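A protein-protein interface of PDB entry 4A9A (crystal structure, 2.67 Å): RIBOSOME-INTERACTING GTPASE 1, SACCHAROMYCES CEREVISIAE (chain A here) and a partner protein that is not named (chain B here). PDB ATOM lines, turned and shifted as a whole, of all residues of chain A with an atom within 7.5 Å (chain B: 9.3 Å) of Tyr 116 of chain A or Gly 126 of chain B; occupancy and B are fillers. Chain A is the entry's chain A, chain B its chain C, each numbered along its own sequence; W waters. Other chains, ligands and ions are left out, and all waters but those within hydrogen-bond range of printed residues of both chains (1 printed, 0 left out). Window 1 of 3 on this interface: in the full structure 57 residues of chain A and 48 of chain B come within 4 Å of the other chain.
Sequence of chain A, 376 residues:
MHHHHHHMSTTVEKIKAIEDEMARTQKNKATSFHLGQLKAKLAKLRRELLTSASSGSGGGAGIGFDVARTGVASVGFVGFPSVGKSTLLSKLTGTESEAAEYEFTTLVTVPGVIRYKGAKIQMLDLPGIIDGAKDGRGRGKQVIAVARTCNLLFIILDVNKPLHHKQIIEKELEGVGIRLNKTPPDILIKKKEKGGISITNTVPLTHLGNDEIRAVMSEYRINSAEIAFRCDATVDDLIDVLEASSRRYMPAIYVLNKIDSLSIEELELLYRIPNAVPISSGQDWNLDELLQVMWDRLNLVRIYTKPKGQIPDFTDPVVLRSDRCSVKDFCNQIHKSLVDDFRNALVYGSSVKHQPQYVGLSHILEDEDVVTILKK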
ATOM      1  N   VAL A  72      21.393  -6.967  16.218  1.00  0.00           N
ATOM      2  CA  VAL A  72      20.765  -5.679  15.910  1.00  0.00           C
ATOM      3  C   VAL A  72      21.807  -4.582  15.717  1.00  0.00           C
ATOM      4  O   VAL A  72      21.534  -3.584  15.070  1.00  0.00           O
ATOM      5  CB  VAL A  72      19.753  -5.206  16.976  1.00  0.00           C
ATOM      6  CG1 VAL A  72      18.510  -6.065  16.947  1.00  0.00           C
ATOM      7  CG2 VAL A  72      20.362  -5.218  18.376  1.00  0.00           C
ATOM      8  N   ILE A 114      27.549 -10.892  21.869  1.00  0.00           N
ATOM      9  CA  ILE A 114      27.010 -10.794  23.232  1.00  0.00           C
ATOM     10  C   ILE A 114      25.538 -10.380  23.239  1.00  0.00           C
ATOM     11  O   ILE A 114      24.977 -10.006  22.203  1.00  0.00           O
ATOM     12  CB  ILE A 114      27.830  -9.865  24.132  1.00  0.00           C
ATOM     13  CG1 ILE A 114      27.747  -8.415  23.627  1.00  0.00           C
ATOM     14  CG2 ILE A 114      29.271 -10.364  24.253  1.00  0.00           C
ATOM     15  CD1 ILE A 114      28.390  -7.441  24.586  1.00  0.00           C
ATOM     16  N   ARG A 115      24.914 -10.499  24.403  1.00  0.00           N
ATOM     17  CA  ARG A 115      23.586  -9.991  24.614  1.00  0.00           C
ATOM     18  C   ARG A 115      23.669  -9.037  25.787  1.00  0.00           C
ATOM     19  O   ARG A 115      24.167  -9.386  26.868  1.00  0.00           O
ATOM     20  CB  ARG A 115      22.590 -11.102  24.908  1.00  0.00           C
ATOM     21  CG  ARG A 115      21.142 -10.616  24.851  1.00  0.00           C
ATOM     22  CD  ARG A 115      20.161 -11.698  25.290  1.00  0.00           C
ATOM     23  NE  ARG A 115      20.063 -12.786  24.319  1.00  0.00           N
ATOM     24  CZ  ARG A 115      19.313 -12.741  23.219  1.00  0.00           C
ATOM     25  NH1 ARG A 115      18.586 -11.659  22.948  1.00  0.00           N
ATOM     26  NH2 ARG A 115      19.295 -13.773  22.383  1.00  0.00           N
ATOM     27  N   TYR A 116      23.189  -7.827  25.545  1.00  0.00           N
ATOM     28  CA  TYR A 116      23.259  -6.751  26.500  1.00  0.00           C
ATOM     29  C   TYR A 116      21.909  -6.074  26.462  1.00  0.00           C
ATOM     30  O   TYR A 116      21.446  -5.672  25.397  1.00  0.00           O
ATOM     31  CB  TYR A 116      24.359  -5.776  26.107  1.00  0.00           C
ATOM     32  CG  TYR A 116      24.743  -4.835  27.209  1.00  0.00           C
ATOM     33  CD1 TYR A 116      25.736  -5.182  28.129  1.00  0.00           C
ATOM     34  CD2 TYR A 116      24.110  -3.596  27.354  1.00  0.00           C
ATOM     35  CE1 TYR A 116      26.087  -4.327  29.153  1.00  0.00           C
ATOM     36  CE2 TYR A 116      24.462  -2.735  28.383  1.00  0.00           C
ATOM     37  CZ  TYR A 116      25.451  -3.109  29.280  1.00  0.00           C
ATOM     38  OH  TYR A 116      25.820  -2.264  30.310  1.00  0.00           O
ATOM     39  N   LYS A 117      21.265  -6.004  27.628  1.00  0.00           N
ATOM     40  CA  LYS A 117      19.923  -5.454  27.783  1.00  0.00           C
ATOM     41  C   LYS A 117      18.985  -5.988  26.719  1.00  0.00           C
ATOM     42  O   LYS A 117      18.137  -5.264  26.201  1.00  0.00           O
ATOM     43  CB  LYS A 117      19.951  -3.932  27.763  1.00  0.00           C
ATOM     44  CG  LYS A 117      20.532  -3.314  29.022  1.00  0.00           C
ATOM     45  CD  LYS A 117      20.910  -1.869  28.740  1.00  0.00           C
ATOM     46  CE  LYS A 117      21.605  -1.182  29.902  1.00  0.00           C
ATOM     47  NZ  LYS A 117      20.591  -0.710  30.859  1.00  0.00           N
ATOM     48  N   GLY A 118      19.133  -7.264  26.390  1.00  0.00           N
ATOM     49  CA  GLY A 118      18.194  -7.905  25.485  1.00  0.00           C
ATOM     50  C   GLY A 118      18.604  -7.811  24.030  1.00  0.00           C
ATOM     51  O   GLY A 118      18.066  -8.515  23.212  1.00  0.00           O
ATOM     52  N   ALA A 119      19.553  -6.944  23.701  1.00  0.00           N
ATOM     53  CA  ALA A 119      20.016  -6.813  22.327  1.00  0.00           C
ATOM     54  C   ALA A 119      21.221  -7.712  22.017  1.00  0.00           C
ATOM     55  O   ALA A 119      22.190  -7.759  22.789  1.00  0.00           O
ATOM     56  CB  ALA A 119      20.356  -5.363  22.035  1.00  0.00           C
ATOM     57  N   LYS A 120      21.153  -8.442  20.905  1.00  0.00           N
ATOM     58  CA  LYS A 120      22.307  -9.189  20.409  1.00  0.00           C
ATOM     59  C   LYS A 120      23.275  -8.235  19.722  1.00  0.00           C
ATOM     60  O   LYS A 120      22.898  -7.538  18.770  1.00  0.00           O
ATOM     61  CB  LYS A 120      21.885 -10.274  19.437  1.00  0.00           C
ATOM     62  CG  LYS A 120      21.403 -11.521  20.125  1.00  0.00           C
ATOM     63  CD  LYS A 120      21.524 -12.733  19.227  1.00  0.00           C
ATOM     64  CE  LYS A 120      20.281 -12.968  18.382  1.00  0.00           C
ATOM     65  NZ  LYS A 120      20.206 -14.389  17.912  1.00  0.00           N
ATOM     66  N   ILE A 121      24.512  -8.176  20.213  1.00  0.00           N
ATOM     67  CA  ILE A 121      25.501  -7.305  19.596  1.00  0.00           C
ATOM     68  C   ILE A 121      26.660  -8.134  19.076  1.00  0.00           C
ATOM     69  O   ILE A 121      27.277  -8.876  19.840  1.00  0.00           O
ATOM     70  CB  ILE A 121      25.985  -6.244  20.565  1.00  0.00           C
ATOM     71  CG1 ILE A 121      24.824  -5.328  20.888  1.00  0.00           C
ATOM     72  CG2 ILE A 121      27.106  -5.422  19.952  1.00  0.00           C
ATOM     73  CD1 ILE A 121      24.950  -4.671  22.237  1.00  0.00           C
ATOM     74  N   LEU A 287      35.468  -2.207  32.825  1.00  0.00           N
ATOM     75  CA  LEU A 287      34.819  -2.986  31.769  1.00  0.00           C
ATOM     76  C   LEU A 287      33.324  -2.784  31.843  1.00  0.00           C
ATOM     77  O   LEU A 287      32.661  -2.701  30.820  1.00  0.00           O
ATOM     78  CB  LEU A 287      35.169  -4.470  31.836  1.00  0.00           C
ATOM     79  CG  LEU A 287      36.656  -4.794  31.650  1.00  0.00           C
ATOM     80  CD1 LEU A 287      36.830  -6.284  31.493  1.00  0.00           C
ATOM     81  CD2 LEU A 287      37.224  -4.065  30.448  1.00  0.00           C
ATOM     82  N   ASP A 288      32.789  -2.654  33.045  1.00  0.00           N
ATOM     83  CA  ASP A 288      31.363  -2.421  33.172  1.00  0.00           C
ATOM     84  C   ASP A 288      31.008  -1.066  32.534  1.00  0.00           C
ATOM     85  O   ASP A 288      30.059  -0.974  31.757  1.00  0.00           O
ATOM     86  CB  ASP A 288      30.894  -2.541  34.624  1.00  0.00           C
ATOM     87  CG  ASP A 288      31.580  -1.563  35.561  1.00  0.00           C
ATOM     88  OD1 ASP A 288      32.544  -0.866  35.150  1.00  0.00           O
ATOM     89  OD2 ASP A 288      31.144  -1.496  36.745  1.00  0.00           O
ATOM     90  N   GLU A 289      31.807  -0.040  32.817  1.00  0.00           N
ATOM     91  CA  GLU A 289      31.609   1.278  32.235  1.00  0.00           C
ATOM     92  C   GLU A 289      31.702   1.215  30.725  1.00  0.00           C
ATOM     93  O   GLU A 289      30.863   1.806  30.043  1.00  0.00           O
ATOM     94  CB  GLU A 289      32.628   2.291  32.774  1.00  0.00           C
ATOM     95  CG  GLU A 289      32.410   3.713  32.278  1.00  0.00           C
ATOM     96  CD  GLU A 289      33.279   4.748  32.973  1.00  0.00           C
ATOM     97  OE1 GLU A 289      34.508   4.591  33.062  1.00  0.00           O
ATOM     98  OE2 GLU A 289      32.727   5.757  33.427  1.00  0.00           O
ATOM     99  N   LEU A 290      32.718   0.508  30.209  1.00  0.00           N
ATOM    100  CA  LEU A 290      32.904   0.348  28.761  1.00  0.00           C
ATOM    101  C   LEU A 290      31.643  -0.142  28.080  1.00  0.00           C
ATOM    102  O   LEU A 290      31.259   0.382  27.036  1.00  0.00           O
ATOM    103  CB  LEU A 290      34.021  -0.634  28.458  1.00  0.00           C
ATOM    104  CG  LEU A 290      34.388  -0.783  26.971  1.00  0.00           C
ATOM    105  CD1 LEU A 290      34.667   0.559  26.302  1.00  0.00           C
ATOM    106  CD2 LEU A 290      35.621  -1.635  26.856  1.00  0.00           C
ATOM    107  N   LEU A 291      30.993  -1.143  28.671  1.00  0.00           N
ATOM    108  CA  LEU A 291      29.807  -1.684  28.069  1.00  0.00           C
ATOM    109  C   LEU A 291      28.642  -0.711  28.199  1.00  0.00           C
ATOM    110  O   LEU A 291      27.871  -0.522  27.249  1.00  0.00           O
ATOM    111  CB  LEU A 291      29.492  -3.054  28.646  1.00  0.00           C
ATOM    112  CG  LEU A 291      30.496  -4.141  28.223  1.00  0.00           C
ATOM    113  CD1 LEU A 291      30.366  -5.368  29.100  1.00  0.00           C
ATOM    114  CD2 LEU A 291      30.361  -4.539  26.759  1.00  0.00           C
ATOM    115  N   GLN A 292      28.529  -0.058  29.351  1.00  0.00           N
ATOM    116  CA  GLN A 292      27.464   0.918  29.541  1.00  0.00           C
ATOM    117  C   GLN A 292      27.548   2.015  28.472  1.00  0.00           C
ATOM    118  O   GLN A 292      26.555   2.349  27.823  1.00  0.00           O
ATOM    119  CB  GLN A 292      27.487   1.503  30.952  1.00  0.00           C
ATOM    120  CG  GLN A 292      26.293   2.415  31.251  1.00  0.00           C
ATOM    121  CD  GLN A 292      24.919   1.727  31.087  1.00  0.00           C
ATOM    122  OE1 GLN A 292      24.583   0.771  31.810  1.00  0.00           O
ATOM    123  NE2 GLN A 292      24.114   2.224  30.134  1.00  0.00           N
ATOM    124  N   VAL A 293      28.746   2.540  28.261  1.00  0.00           N
ATOM    125  CA  VAL A 293      28.937   3.610  27.313  1.00  0.00           C
ATOM    126  C   VAL A 293      28.640   3.113  25.901  1.00  0.00           C
ATOM    127  O   VAL A 293      27.987   3.793  25.111  1.00  0.00           O
ATOM    128  CB  VAL A 293      30.355   4.185  27.441  1.00  0.00           C
ATOM    129  CG1 VAL A 293      30.700   5.104  26.271  1.00  0.00           C
ATOM    130  CG2 VAL A 293      30.490   4.918  28.771  1.00  0.00           C
ATOM    131  N   MET A 294      29.078   1.898  25.604  1.00  0.00           N
ATOM    132  CA  MET A 294      28.775   1.316  24.315  1.00  0.00           C
ATOM    133  C   MET A 294      27.264   1.345  24.093  1.00  0.00           C
ATOM    134  O   MET A 294      26.779   1.846  23.077  1.00  0.00           O
ATOM    135  CB  MET A 294      29.311  -0.109  24.221  1.00  0.00           C
ATOM    136  CG  MET A 294      28.822  -0.861  22.994  1.00  0.00           C
ATOM    137  SD  MET A 294      28.922  -2.646  23.203  1.00  0.00           S
ATOM    138  CE  MET A 294      27.576  -2.933  24.356  1.00  0.00           C
ATOM    139  N   TRP A 295      26.518   0.822  25.054  1.00  0.00           N
ATOM    140  CA  TRP A 295      25.073   0.825  24.946  1.00  0.00           C
ATOM    141  C   TRP A 295      24.523   2.214  24.713  1.00  0.00           C
ATOM    142  O   TRP A 295      23.688   2.415  23.831  1.00  0.00           O
ATOM    143  CB  TRP A 295      24.455   0.201  26.180  1.00  0.00           C
ATOM    144  CG  TRP A 295      22.962   0.306  26.165  1.00  0.00           C
ATOM    145  CD1 TRP A 295      22.175   1.260  26.794  1.00  0.00           C
ATOM    146  CD2 TRP A 295      22.022  -0.562  25.453  1.00  0.00           C
ATOM    147  NE1 TRP A 295      20.861   1.042  26.527  1.00  0.00           N
ATOM    148  CE2 TRP A 295      20.696  -0.037  25.735  1.00  0.00           C
ATOM    149  CE3 TRP A 295      22.147  -1.685  24.638  1.00  0.00           C
ATOM    150  CZ2 TRP A 295      19.553  -0.621  25.220  1.00  0.00           C
ATOM    151  CZ3 TRP A 295      20.990  -2.267  24.123  1.00  0.00           C
ATOM    152  CH2 TRP A 295      19.724  -1.751  24.414  1.00  0.00           C
ATOM    153  N   ASP A 296      24.984   3.180  25.501  1.00  0.00           N
ATOM    154  CA  ASP A 296      24.537   4.564  25.361  1.00  0.00           C
ATOM    155  C   ASP A 296      24.749   5.119  23.953  1.00  0.00           C
ATOM    156  O   ASP A 296      23.880   5.820  23.438  1.00  0.00           O
ATOM    157  CB  ASP A 296      25.244   5.473  26.371  1.00  0.00           C
ATOM    158  CG  ASP A 296      24.789   5.237  27.803  1.00  0.00           C
ATOM    159  OD1 ASP A 296      23.679   4.707  28.013  1.00  0.00           O
ATOM    160  OD2 ASP A 296      25.546   5.594  28.740  1.00  0.00           O
ATOM    161  N   LEU A 298      25.072   3.452  21.102  1.00  0.00           N
ATOM    162  CA  LEU A 298      24.468   2.670  20.032  1.00  0.00           C
ATOM    163  C   LEU A 298      23.031   3.101  19.775  1.00  0.00           C
ATOM    164  O   LEU A 298      22.499   2.851  18.691  1.00  0.00           O
ATOM    165  CB  LEU A 298      24.488   1.190  20.373  1.00  0.00           C
ATOM    166  CG  LEU A 298      25.763   0.388  20.138  1.00  0.00           C
ATOM    167  CD1 LEU A 298      25.582  -1.018  20.672  1.00  0.00           C
ATOM    168  CD2 LEU A 298      26.096   0.344  18.658  1.00  0.00           C
ATOM    169  N   LEU A 300      20.023   2.042  20.561  1.00  0.00           N
ATOM    170  CA  LEU A 300      19.059   1.058  20.069  1.00  0.00           C
ATOM    171  C   LEU A 300      17.690   1.325  20.682  1.00  0.00           C
ATOM    172  O   LEU A 300      17.604   1.981  21.731  1.00  0.00           O
ATOM    173  CB  LEU A 300      19.536  -0.356  20.397  1.00  0.00           C
ATOM    174  CG  LEU A 300      20.893  -0.734  19.786  1.00  0.00           C
ATOM    175  CD1 LEU A 300      21.405  -2.027  20.404  1.00  0.00           C
ATOM    176  CD2 LEU A 300      20.826  -0.850  18.270  1.00  0.00           C
ATOM    177  N   ARG A 302      14.412  -0.467  22.257  1.00  0.00           N
ATOM    178  CA  ARG A 302      13.628  -1.581  22.766  1.00  0.00           C
ATOM    179  C   ARG A 302      12.164  -1.232  22.766  1.00  0.00           C
ATOM    180  O   ARG A 302      11.771  -0.233  23.358  1.00  0.00           O
ATOM    181  CB  ARG A 302      14.035  -1.879  24.195  1.00  0.00           C
ATOM    182  CG  ARG A 302      15.462  -2.349  24.317  1.00  0.00           C
ATOM    183  CD  ARG A 302      15.901  -2.203  25.740  1.00  0.00           C
ATOM    184  NE  ARG A 302      16.180  -0.814  26.050  1.00  0.00           N
ATOM    185  CZ  ARG A 302      16.497  -0.392  27.266  1.00  0.00           C
ATOM    186  NH1 ARG A 302      16.574  -1.262  28.264  1.00  0.00           N
ATOM    187  NH2 ARG A 302      16.746   0.890  27.477  1.00  0.00           N
ATOM    188  N   VAL A 319      14.189  -5.399  19.700  1.00  0.00           N
ATOM    189  CA  VAL A 319      15.158  -4.336  19.628  1.00  0.00           C
ATOM    190  C   VAL A 319      15.334  -3.906  18.188  1.00  0.00           C
ATOM    191  O   VAL A 319      15.625  -4.720  17.315  1.00  0.00           O
ATOM    192  CB  VAL A 319      16.493  -4.755  20.242  1.00  0.00           C
ATOM    193  CG1 VAL A 319      17.421  -3.555  20.313  1.00  0.00           C
ATOM    194  CG2 VAL A 319      16.270  -5.330  21.630  1.00  0.00           C
ATOM    195  N   ASP B 117      21.670 -19.208  21.977  1.00  0.00           N
ATOM    196  CA  ASP B 117      22.095 -18.665  23.274  1.00  0.00           C
ATOM    197  C   ASP B 117      23.303 -19.343  23.919  1.00  0.00           C
ATOM    198  O   ASP B 117      24.034 -18.703  24.667  1.00  0.00           O
ATOM    199  CB  ASP B 117      20.928 -18.615  24.266  1.00  0.00           C
ATOM    200  CG  ASP B 117      20.096 -17.338  24.140  1.00  0.00           C
ATOM    201  OD1 ASP B 117      20.475 -16.404  23.385  1.00  0.00           O
ATOM    202  OD2 ASP B 117      19.044 -17.274  24.818  1.00  0.00           O
ATOM    203  N   ILE B 120      26.557 -17.477  23.260  1.00  0.00           N
ATOM    204  CA  ILE B 120      26.438 -16.036  23.429  1.00  0.00           C
ATOM    205  C   ILE B 120      26.405 -15.689  24.910  1.00  0.00           C
ATOM    206  O   ILE B 120      25.544 -16.181  25.646  1.00  0.00           O
ATOM    207  CB  ILE B 120      25.155 -15.510  22.761  1.00  0.00           C
ATOM    208  CG1 ILE B 120      25.276 -15.582  21.231  1.00  0.00           C
ATOM    209  CG2 ILE B 120      24.860 -14.094  23.228  1.00  0.00           C
ATOM    210  CD1 ILE B 120      23.981 -15.313  20.481  1.00  0.00           C
ATOM    211  N   LYS B 121      27.350 -14.857  25.341  1.00  0.00           N
ATOM    212  CA  LYS B 121      27.400 -14.361  26.704  1.00  0.00           C
ATOM    213  C   LYS B 121      26.307 -13.322  26.946  1.00  0.00           C
ATOM    214  O   LYS B 121      26.214 -12.320  26.229  1.00  0.00           O
ATOM    215  CB  LYS B 121      28.753 -13.738  26.995  1.00  0.00           C
ATOM    216  CG  LYS B 121      28.937 -13.402  28.459  1.00  0.00           C
ATOM    217  CD  LYS B 121      30.054 -12.393  28.709  1.00  0.00           C
ATOM    218  CE  LYS B 121      30.240 -12.178  30.210  1.00  0.00           C
ATOM    219  NZ  LYS B 121      31.558 -11.564  30.486  1.00  0.00           N
ATOM    220  N   ASP B 122      25.497 -13.560  27.970  1.00  0.00           N
ATOM    221  CA  ASP B 122      24.398 -12.675  28.298  1.00  0.00           C
ATOM    222  C   ASP B 122      24.736 -11.809  29.501  1.00  0.00           C
ATOM    223  O   ASP B 122      24.909 -12.306  30.603  1.00  0.00           O
ATOM    224  CB  ASP B 122      23.136 -13.482  28.598  1.00  0.00           C
ATOM    225  CG  ASP B 122      21.893 -12.613  28.657  1.00  0.00           C
ATOM    226  OD1 ASP B 122      21.984 -11.370  28.479  1.00  0.00           O
ATOM    227  OD2 ASP B 122      20.807 -13.176  28.875  1.00  0.00           O
ATOM    228  N   TYR B 123      24.806 -10.508  29.277  1.00  0.00           N
ATOM    229  CA  TYR B 123      25.088  -9.553  30.333  1.00  0.00           C
ATOM    230  C   TYR B 123      23.828  -9.112  31.093  1.00  0.00           C
ATOM    231  O   TYR B 123      23.901  -8.259  31.992  1.00  0.00           O
ATOM    232  CB  TYR B 123      25.770  -8.333  29.724  1.00  0.00           C
ATOM    233  CG  TYR B 123      27.216  -8.563  29.426  1.00  0.00           C
ATOM    234  CD1 TYR B 123      28.173  -8.506  30.445  1.00  0.00           C
ATOM    235  CD2 TYR B 123      27.641  -8.857  28.127  1.00  0.00           C
ATOM    236  CE1 TYR B 123      29.509  -8.726  30.170  1.00  0.00           C
ATOM    237  CE2 TYR B 123      28.977  -9.073  27.845  1.00  0.00           C
ATOM    238  CZ  TYR B 123      29.906  -9.006  28.871  1.00  0.00           C
ATOM    239  OH  TYR B 123      31.242  -9.228  28.599  1.00  0.00           O
ATOM    240  N   GLY B 124      22.681  -9.688  30.731  1.00  0.00           N
ATOM    241  CA  GLY B 124      21.419  -9.315  31.353  1.00  0.00           C
ATOM    242  C   GLY B 124      21.205  -7.820  31.261  1.00  0.00           C
ATOM    243  O   GLY B 124      21.275  -7.251  30.171  1.00  0.00           O
ATOM    244  N   ASP B 125      20.963  -7.183  32.403  1.00  0.00           N
ATOM    245  CA  ASP B 125      20.641  -5.749  32.435  1.00  0.00           C
ATOM    246  C   ASP B 125      21.894  -4.874  32.495  1.00  0.00           C
ATOM    247  O   ASP B 125      21.803  -3.648  32.598  1.00  0.00           O
ATOM    248  CB  ASP B 125      19.688  -5.413  33.595  1.00  0.00           C
ATOM    249  CG  ASP B 125      20.342  -5.550  34.982  1.00  0.00           C
ATOM    250  OD1 ASP B 125      21.543  -5.901  35.112  1.00  0.00           O
ATOM    251  OD2 ASP B 125      19.636  -5.300  35.977  1.00  0.00           O
ATOM    252  N   GLY B 126      23.054  -5.515  32.457  1.00  0.00           N
ATOM    253  CA  GLY B 126      24.308  -4.798  32.467  1.00  0.00           C
ATOM    254  C   GLY B 126      24.837  -4.443  33.840  1.00  0.00           C
ATOM    255  O   GLY B 126      25.923  -3.868  33.951  1.00  0.00           O
ATOM    256  N   SER B 127      24.106  -4.766  34.900  1.00  0.00           N
ATOM    257  CA  SER B 127      24.651  -4.504  36.238  1.00  0.00           C
ATOM    258  C   SER B 127      25.610  -5.615  36.682  1.00  0.00           C
ATOM    259  O   SER B 127      25.450  -6.788  36.305  1.00  0.00           O
ATOM    260  CB  SER B 127      23.551  -4.276  37.273  1.00  0.00           C
ATOM    261  OG  SER B 127      22.742  -5.424  37.377  1.00  0.00           O
ATOM    262  N   ASN B 128      26.608  -5.218  37.471  1.00  0.00           N
ATOM    263  CA  ASN B 128      27.617  -6.130  38.018  1.00  0.00           C
ATOM    264  C   ASN B 128      28.065  -7.250  37.084  1.00  0.00           C
ATOM    265  O   ASN B 128      27.855  -8.423  37.375  1.00  0.00           O
ATOM    266  CB  ASN B 128      27.136  -6.705  39.347  1.00  0.00           C
ATOM    267  CG  ASN B 128      27.062  -5.651  40.416  1.00  0.00           C
ATOM    268  OD1 ASN B 128      25.984  -5.153  40.736  1.00  0.00           O
ATOM    269  ND2 ASN B 128      28.220  -5.271  40.952  1.00  0.00           N
ATOM    270  N   PRO B 129      28.673  -6.893  35.950  1.00  0.00           N
ATOM    271  CA  PRO B 129      29.072  -7.963  35.040  1.00  0.00           C
ATOM    272  C   PRO B 129      30.309  -8.689  35.568  1.00  0.00           C
ATOM    273  O   PRO B 129      31.057  -8.115  36.367  1.00  0.00           O
ATOM    274  CB  PRO B 129      29.377  -7.219  33.745  1.00  0.00           C
ATOM    275  CG  PRO B 129      29.697  -5.817  34.148  1.00  0.00           C
ATOM    276  CD  PRO B 129      29.004  -5.545  35.444  1.00  0.00           C
ATOM    277  N   THR B 130      30.498  -9.945  35.161  1.00  0.00           N
ATOM    278  CA  THR B 130      31.703 -10.704  35.486  1.00  0.00           C
ATOM    279  C   THR B 130      32.360 -11.071  34.169  1.00  0.00           C
ATOM    280  O   THR B 130      31.706 -11.070  33.123  1.00  0.00           O
ATOM    281  CB  THR B 130      31.403 -12.026  36.213  1.00  0.00           C
ATOM    282  OG1 THR B 130      30.491 -12.797  35.417  1.00  0.00           O
ATOM    283  CG2 THR B 130      30.826 -11.797  37.609  1.00  0.00           C
ATOM    284  N   PHE B 131      33.645 -11.416  34.234  1.00  0.00           N
ATOM    285  CA  PHE B 131      34.457 -11.565  33.058  1.00  0.00           C
ATOM    286  C   PHE B 131      35.306 -12.831  33.031  1.00  0.00           C
ATOM    287  O   PHE B 131      36.479 -12.801  32.663  1.00  0.00           O
ATOM    288  CB  PHE B 131      35.292 -10.290  32.890  1.00  0.00           C
ATOM    289  CG  PHE B 131      34.447  -9.063  32.747  1.00  0.00           C
ATOM    290  CD1 PHE B 131      33.922  -8.712  31.501  1.00  0.00           C
ATOM    291  CD2 PHE B 131      34.122  -8.298  33.852  1.00  0.00           C
ATOM    292  CE1 PHE B 131      33.100  -7.601  31.358  1.00  0.00           C
ATOM    293  CE2 PHE B 131      33.312  -7.184  33.718  1.00  0.00           C
ATOM    294  CZ  PHE B 131      32.800  -6.832  32.467  1.00  0.00           C
HETATM  295  O   HOH W   1      20.303  -9.206  27.992  1.00  0.00           O
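O of Lys 120 of chain A sits at hydrogen-bond distance from N of Val 72 of chain A (3.0 Å).
The side-chain hydroxyl (OH) of Tyr 123 of chain B sits at hydrogen-bond distance from the side-chain amino group (NZ) of Lys 121 of chain B (3.0 Å).
The backbone carbonyl oxygen (O) of Thr 130 of chain B lies within hydrogen-bond range of the side-chain amino group (NZ) of Lys 121 of chain B (2.7 Å).
The side-chain carboxylate (OD1) of Asp 125 of chain B lies within hydrogen-bond range of the side-chain hydroxyl (OG) of Ser 127 of chain B.
The side-chain carboxylate of Asp 117 of chain B is in salt-bridge range of the guanidinium group of Arg 115 of chain A.
The backbone carbonyl oxygen (O) of Lys 121 of chain B is in hydrogen-bond range of the backbone NH (N) of Arg 115 of chain A, at 2.9 Å.
N of Tyr 123 of chain B lies within hydrogen-bond range of O of Arg 115 of chain A, at 2.7 Å.
O of Gly 124 of chain B is in hydrogen-bond range of N of Lys 117 of chain A (2.8 Å).
The side-chain carboxylate of Asp 122 of chain B lies close to the backbone carbonyl oxygen of Arg 115 of chain A, 3.4 Å away.
Water W1 lies within hydrogen-bond range of the backbone NH of Gly 118 of chain A (2.8 Å), the side-chain carboxylate of Asp 122 of chain B (2.8 Å), the backbone carbonyl oxygen of Gly 124 of chain B (3.1 Å) and the backbone NH of Lys 117 of chain A (3.4 Å).
Of the 13 printed residues of chain B, 10 touch a printed residue of chain A.
Printed residues of chain B that touch a printed residue of chain A: Asp 117, Ile 120, Lys 121, Asp 122, Tyr 123, Gly 124, Asp 125, Gly 126, Pro 129 and Phe 131.
Hydrophobic or aromatic side chains of chain B that line the printed part of chain A: Ile 120, Tyr 123, Pro 129 and Phe 131.
Ile 120 of chain B touches Ile 114 of chain A (CG2 to C, 3.8 Å).
Ile 114 of chain A touches Lys 121 of chain B.
Ile 114 of chain A touches Tyr 123 of chain B.
Arg 115 of chain A touches Ile 120 of chain B (N to CG2, 3.8 Å).
CB of Tyr 123 of chain B touches CD1 of Tyr 116 of chain A (3.5 Å).
C of Tyr 116 of chain A touches O of Gly 124 of chain B, at 3.9 Å.
Tyr 116 of chain A touches Gly 126 of chain B (OH to CA, 3.7 Å).
Lys 117 of chain A touches Asp 125 of chain B.
Lys 120 of chain A touches Ile 120 of chain B (CD to CD1, 3.8 Å).
Tyr 123 of chain B touches Leu 291 of chain A.
Tyr 116 of chain A touches just these residues of chain B: Tyr 123, Gly 124 and Gly 126.
Gly 118 of chain A touches none of the printed residues of chain B.
Ala 119 of chain A touches none of the printed residues of chain B.
Of the printed residues of chain B, Asp 288 of chain A touches Pro 129.
Asp 296 of chain A touches none of the printed residues of chain B.
Of the printed residues of chain A, Asp 122 of chain B touches Arg 115 (3.4 Å).
Printed residues of chain A within 4 Å of Gly 124 of chain B: Tyr 116 and Lys 117.
Printed residues of chain A within 4 Å of Asp 125 of chain B: Lys 117.
Gly 126 of chain B touches one residue of chain A.
Of the printed residues of chain A, Phe 131 of chain B touches Leu 287 (3.4 Å).
The nearest residue of chain A that does not touch Gly 126 of chain B is Lys 117 of chain A (4.8 Å).
The nearest printed residue of chain B that does not touch Lys 120 of chain A is Asp 117 of chain B (5.6 Å).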
